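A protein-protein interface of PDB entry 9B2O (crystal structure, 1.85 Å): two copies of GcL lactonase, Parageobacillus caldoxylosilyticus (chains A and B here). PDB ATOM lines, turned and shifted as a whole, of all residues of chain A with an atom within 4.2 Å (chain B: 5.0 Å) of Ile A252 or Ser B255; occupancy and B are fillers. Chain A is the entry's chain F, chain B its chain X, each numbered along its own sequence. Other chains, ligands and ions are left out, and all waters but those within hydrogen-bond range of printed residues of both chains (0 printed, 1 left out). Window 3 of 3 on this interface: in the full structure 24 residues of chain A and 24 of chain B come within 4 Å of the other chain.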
ATOM      1  N   GLY A 211      -6.330 -11.700   6.745  1.00  0.00           N
ATOM      2  CA  GLY A 211      -5.373 -11.612   5.640  1.00  0.00           C
ATOM      3  C   GLY A 211      -3.989 -11.755   6.201  1.00  0.00           C
ATOM      4  O   GLY A 211      -3.617 -12.859   6.586  1.00  0.00           O
ATOM      5  N   PRO A 249       3.371 -11.255   1.319  1.00  0.00           N
ATOM      6  CA  PRO A 249       4.383 -11.572   2.321  1.00  0.00           C
ATOM      7  C   PRO A 249       4.646 -13.080   2.506  1.00  0.00           C
ATOM      8  O   PRO A 249       3.840 -13.911   2.055  1.00  0.00           O
ATOM      9  CB  PRO A 249       3.792 -10.923   3.589  1.00  0.00           C
ATOM     10  CG  PRO A 249       2.300 -10.952   3.373  1.00  0.00           C
ATOM     11  CD  PRO A 249       2.152 -10.661   1.901  1.00  0.00           C
ATOM     12  N   ILE A 251       4.895 -15.072   5.081  1.00  0.00           N
ATOM     13  CA  ILE A 251       3.926 -15.829   5.905  1.00  0.00           C
ATOM     14  C   ILE A 251       2.641 -14.993   5.945  1.00  0.00           C
ATOM     15  O   ILE A 251       2.679 -13.731   5.880  1.00  0.00           O
ATOM     16  CB  ILE A 251       4.529 -16.157   7.288  1.00  0.00           C
ATOM     17  CG1 ILE A 251       3.909 -17.411   7.931  1.00  0.00           C
ATOM     18  CG2 ILE A 251       4.482 -14.911   8.187  1.00  0.00           C
ATOM     19  CD1 ILE A 251       2.886 -17.140   9.035  1.00  0.00           C
ATOM     20  N   ILE A 252       1.517 -15.678   6.062  1.00  0.00           N
ATOM     21  CA  ILE A 252       0.206 -15.012   5.917  1.00  0.00           C
ATOM     22  C   ILE A 252      -0.789 -15.847   6.704  1.00  0.00           C
ATOM     23  O   ILE A 252      -0.655 -17.059   6.671  1.00  0.00           O
ATOM     24  CB  ILE A 252      -0.038 -14.985   4.404  1.00  0.00           C
ATOM     25  CG1 ILE A 252      -0.947 -13.851   3.955  1.00  0.00           C
ATOM     26  CG2 ILE A 252      -0.504 -16.342   3.914  1.00  0.00           C
ATOM     27  CD1 ILE A 252      -0.691 -13.509   2.505  1.00  0.00           C
ATOM     28  N   TYR A 253      -1.761 -15.245   7.367  1.00  0.00           N
ATOM     29  CA  TYR A 253      -2.822 -16.053   7.993  1.00  0.00           C
ATOM     30  C   TYR A 253      -3.793 -16.546   6.899  1.00  0.00           C
ATOM     31  O   TYR A 253      -4.041 -17.764   6.814  1.00  0.00           O
ATOM     32  CB  TYR A 253      -3.571 -15.280   9.077  1.00  0.00           C
ATOM     33  CG  TYR A 253      -4.757 -16.051   9.549  1.00  0.00           C
ATOM     34  CD1 TYR A 253      -4.614 -17.297  10.168  1.00  0.00           C
ATOM     35  CD2 TYR A 253      -6.034 -15.551   9.361  1.00  0.00           C
ATOM     36  CE1 TYR A 253      -5.725 -18.019  10.605  1.00  0.00           C
ATOM     37  CE2 TYR A 253      -7.137 -16.263   9.792  1.00  0.00           C
ATOM     38  CZ  TYR A 253      -6.986 -17.493  10.407  1.00  0.00           C
ATOM     39  OH  TYR A 253      -8.123 -18.148  10.783  1.00  0.00           O
ATOM     40  N   ASP A 254      -4.366 -15.628   6.107  1.00  0.00           N
ATOM     41  CA  ASP A 254      -5.434 -15.921   5.117  1.00  0.00           C
ATOM     42  C   ASP A 254      -5.023 -15.372   3.747  1.00  0.00           C
ATOM     43  O   ASP A 254      -5.178 -14.184   3.533  1.00  0.00           O
ATOM     44  CB  ASP A 254      -6.740 -15.288   5.606  1.00  0.00           C
ATOM     45  CG  ASP A 254      -7.892 -15.401   4.627  1.00  0.00           C
ATOM     46  OD1 ASP A 254      -7.750 -16.137   3.630  1.00  0.00           O
ATOM     47  OD2 ASP A 254      -8.915 -14.705   4.855  1.00  0.00           O
ATOM     48  N   SER A 255      -4.400 -16.162   2.892  1.00  0.00           N
ATOM     49  CA  SER A 255      -3.791 -15.660   1.630  1.00  0.00           C
ATOM     50  C   SER A 255      -4.894 -15.063   0.755  1.00  0.00           C
ATOM     51  O   SER A 255      -4.671 -14.011   0.164  1.00  0.00           O
ATOM     52  CB  SER A 255      -3.041 -16.735   0.896  1.00  0.00           C
ATOM     53  OG  SER A 255      -3.866 -17.882   0.710  1.00  0.00           O
ATOM     54  N   TYR A 258      -6.027 -11.742   2.155  1.00  0.00           N
ATOM     55  CA  TYR A 258      -4.918 -10.789   1.928  1.00  0.00           C
ATOM     56  C   TYR A 258      -5.053 -10.215   0.504  1.00  0.00           C
ATOM     57  O   TYR A 258      -5.097  -9.002   0.292  1.00  0.00           O
ATOM     58  CB  TYR A 258      -3.553 -11.448   2.141  1.00  0.00           C
ATOM     59  CG  TYR A 258      -2.403 -10.570   1.708  1.00  0.00           C
ATOM     60  CD1 TYR A 258      -1.861  -9.647   2.593  1.00  0.00           C
ATOM     61  CD2 TYR A 258      -1.956 -10.554   0.398  1.00  0.00           C
ATOM     62  CE1 TYR A 258      -0.875  -8.758   2.203  1.00  0.00           C
ATOM     63  CE2 TYR A 258      -0.952  -9.680  -0.002  1.00  0.00           C
ATOM     64  CZ  TYR A 258      -0.440  -8.758   0.895  1.00  0.00           C
ATOM     65  OH  TYR A 258       0.526  -7.882   0.537  1.00  0.00           O
ATOM     66  N   GLY B 211      -6.166 -25.028  -1.673  1.00  0.00           N
ATOM     67  CA  GLY B 211      -5.124 -25.029  -0.652  1.00  0.00           C
ATOM     68  C   GLY B 211      -3.788 -24.765  -1.290  1.00  0.00           C
ATOM     69  O   GLY B 211      -3.535 -23.615  -1.674  1.00  0.00           O
ATOM     70  N   ILE B 252       1.429 -20.485  -1.519  1.00  0.00           N
ATOM     71  CA  ILE B 252       0.185 -21.238  -1.259  1.00  0.00           C
ATOM     72  C   ILE B 252      -0.917 -20.484  -1.994  1.00  0.00           C
ATOM     73  O   ILE B 252      -0.891 -19.261  -1.940  1.00  0.00           O
ATOM     74  CB  ILE B 252       0.044 -21.264   0.276  1.00  0.00           C
ATOM     75  CG1 ILE B 252      -0.739 -22.465   0.793  1.00  0.00           C
ATOM     76  CG2 ILE B 252      -0.512 -19.948   0.798  1.00  0.00           C
ATOM     77  CD1 ILE B 252      -0.350 -22.814   2.221  1.00  0.00           C
ATOM     78  N   TYR B 253      -1.877 -21.155  -2.619  1.00  0.00           N
ATOM     79  CA  TYR B 253      -3.040 -20.410  -3.135  1.00  0.00           C
ATOM     80  C   TYR B 253      -3.956 -20.002  -1.957  1.00  0.00           C
ATOM     81  O   TYR B 253      -4.255 -18.803  -1.833  1.00  0.00           O
ATOM     82  CB  TYR B 253      -3.800 -21.203  -4.195  1.00  0.00           C
ATOM     83  CG  TYR B 253      -5.083 -20.529  -4.566  1.00  0.00           C
ATOM     84  CD1 TYR B 253      -5.078 -19.301  -5.235  1.00  0.00           C
ATOM     85  CD2 TYR B 253      -6.297 -21.106  -4.255  1.00  0.00           C
ATOM     86  CE1 TYR B 253      -6.259 -18.660  -5.588  1.00  0.00           C
ATOM     87  CE2 TYR B 253      -7.479 -20.466  -4.569  1.00  0.00           C
ATOM     88  CZ  TYR B 253      -7.463 -19.267  -5.258  1.00  0.00           C
ATOM     89  OH  TYR B 253      -8.670 -18.705  -5.546  1.00  0.00           O
ATOM     90  N   ASP B 254      -4.457 -20.962  -1.167  1.00  0.00           N
ATOM     91  CA  ASP B 254      -5.456 -20.725  -0.097  1.00  0.00           C
ATOM     92  C   ASP B 254      -4.868 -21.226   1.224  1.00  0.00           C
ATOM     93  O   ASP B 254      -4.963 -22.437   1.499  1.00  0.00           O
ATOM     94  CB  ASP B 254      -6.754 -21.444  -0.481  1.00  0.00           C
ATOM     95  CG  ASP B 254      -7.854 -21.420   0.565  1.00  0.00           C
ATOM     96  OD1 ASP B 254      -7.721 -20.657   1.536  1.00  0.00           O
ATOM     97  OD2 ASP B 254      -8.831 -22.208   0.423  1.00  0.00           O
ATOM     98  N   SER B 255      -4.200 -20.389   1.996  1.00  0.00           N
ATOM     99  CA  SER B 255      -3.552 -20.838   3.258  1.00  0.00           C
ATOM    100  C   SER B 255      -4.576 -21.506   4.190  1.00  0.00           C
ATOM    101  O   SER B 255      -4.224 -22.525   4.785  1.00  0.00           O
ATOM    102  CB  SER B 255      -2.844 -19.710   3.972  1.00  0.00           C
ATOM    103  OG  SER B 255      -3.745 -18.643   4.238  1.00  0.00           O
ATOM    104  N   LEU B 256      -5.774 -20.946   4.380  1.00  0.00           N
ATOM    105  CA  LEU B 256      -6.785 -21.472   5.330  1.00  0.00           C
ATOM    106  C   LEU B 256      -7.194 -22.859   4.844  1.00  0.00           C
ATOM    107  O   LEU B 256      -7.274 -23.793   5.682  1.00  0.00           O
ATOM    108  CB  LEU B 256      -7.998 -20.536   5.438  1.00  0.00           C
ATOM    109  CG  LEU B 256      -7.751 -19.224   6.203  1.00  0.00           C
ATOM    110  CD1 LEU B 256      -9.060 -18.434   6.381  1.00  0.00           C
ATOM    111  CD2 LEU B 256      -7.125 -19.471   7.579  1.00  0.00           C
ATOM    112  N   GLY B 257      -7.468 -22.991   3.541  1.00  0.00           N
ATOM    113  CA  GLY B 257      -7.880 -24.290   2.973  1.00  0.00           C
ATOM    114  C   GLY B 257      -6.769 -25.325   3.098  1.00  0.00           C
ATOM    115  O   GLY B 257      -7.058 -26.501   3.375  1.00  0.00           O
ATOM    116  N   TYR B 258      -5.536 -24.904   2.920  1.00  0.00           N
ATOM    117  CA  TYR B 258      -4.355 -25.784   3.070  1.00  0.00           C
ATOM    118  C   TYR B 258      -4.360 -26.366   4.491  1.00  0.00           C
ATOM    119  O   TYR B 258      -4.319 -27.581   4.667  1.00  0.00           O
ATOM    120  CB  TYR B 258      -3.050 -25.036   2.769  1.00  0.00           C
ATOM    121  CG  TYR B 258      -1.838 -25.877   3.071  1.00  0.00           C
ATOM    122  CD1 TYR B 258      -1.321 -26.763   2.129  1.00  0.00           C
ATOM    123  CD2 TYR B 258      -1.269 -25.851   4.326  1.00  0.00           C
ATOM    124  CE1 TYR B 258      -0.264 -27.607   2.431  1.00  0.00           C
ATOM    125  CE2 TYR B 258      -0.202 -26.678   4.632  1.00  0.00           C
ATOM    126  CZ  TYR B 258       0.305 -27.550   3.685  1.00  0.00           C
ATOM    127  OH  TYR B 258       1.340 -28.357   4.034  1.00  0.00           O
ATOM    128  N   MET B 259      -4.411 -25.494   5.495  1.00  0.00           N
ATOM    129  CA  MET B 259      -4.328 -25.899   6.933  1.00  0.00           C
ATOM    130  C   MET B 259      -5.524 -26.800   7.261  1.00  0.00           C
ATOM    131  O   MET B 259      -5.310 -27.822   7.937  1.00  0.00           O
ATOM    132  CB  MET B 259      -4.347 -24.678   7.867  1.00  0.00           C
ATOM    133  CG  MET B 259      -3.182 -23.729   7.672  1.00  0.00           C
ATOM    134  SD  MET B 259      -1.571 -24.522   7.923  1.00  0.00           S
ATOM    135  CE  MET B 259      -1.650 -24.709   9.703  1.00  0.00           C
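Of the 8 printed residues of chain A, 4 touch a printed residue of chain B.
Hydrophobic or aromatic side chains of chain A within 4 Å of the printed part of chain B: Ile A252 and Tyr A253.
Of the 9 printed residues of chain B, 5 touch a printed residue of chain A.
O of Gly A211 sits at hydrogen-bond distance from N of Tyr A253, 3.1 Å away.
The backbone carbonyl oxygen (O) of Gly B211 sits at hydrogen-bond distance from the backbone NH (N) of Asp B254 (2.9 Å).
The backbone NH of Tyr B253 is in hydrogen-bond range of the backbone carbonyl oxygen of Gly B211 (3.1 Å).
The side-chain carboxylate of Asp B254 sits at hydrogen-bond distance from the backbone NH of Gly B257 (3.1 Å).
The backbone carbonyl oxygen (O) of Gly A211 lies within hydrogen-bond range of the backbone NH (N) of Asp A254 (2.9 Å).
The side-chain carboxylate (OD1) of Asp B254 sits close to the backbone NH (N) of Leu B256, 3.5 Å away.
CG2 of Ile A252 touches OG of Ser B255 (3.99 Å).
Leu B256 touches Tyr A253 (CD2 to CZ, 3.5 Å).
CA of Asp A254 touches OG of Ser B255 (3.3 Å).
CG of Asp A254 touches CD1 of Leu B256, 3.7 Å away.
Ile B252 touches Ser A255 (CG2 to OG, 3.9 Å).
Asp B254 touches Ser A255.
O of Tyr B253 lies within hydrogen-bond range of OG of Ser A255.
The backbone NH of Ser B255 lies within hydrogen-bond range of the side-chain hydroxyl of Ser A255 (2.8 Å).
The side-chain hydroxyl of Ser B255 is in hydrogen-bond range of the backbone carbonyl oxygen of Tyr A253 (2.7 Å).
Printed residues of chain B within 4 Å of Ile A252: Ser B255.
Printed residues of chain A within 4 Å of Ser B255: Ile A252, Tyr A253, Asp A254 and Ser A255.
Of the printed residues of chain B, Ser A255 touches Ile B252 (3.9 Å), Tyr B253 (2.7 Å), Asp B254 (3.4 Å) and Ser B255 (2.8 Å).
Of the printed residues of chain B, Asp A254 touches Ser B255 and Leu B256.
Printed residues of chain A within 4 Å of Tyr B253: Ser A255.
The nearest printed residue of chain A that does not touch Ser B255 is Gly A211 (6.2 Å).
Ile A252 touches Ser B255, and with the chains exchanged Ser A255 touches Ile B252.
Tyr A253 touches Ser B255, and with the chains exchanged Ser A255 touches Tyr B253.
Asp A254 touches Ser B255, and with the chains exchanged Ser A255 touches Asp B254.
Ser B255 touches its own counterpart, Ser A255.
Of the 9 pairs that touch across the chains among the printed residues, 7 have their exchanged pair printed and touching as well.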
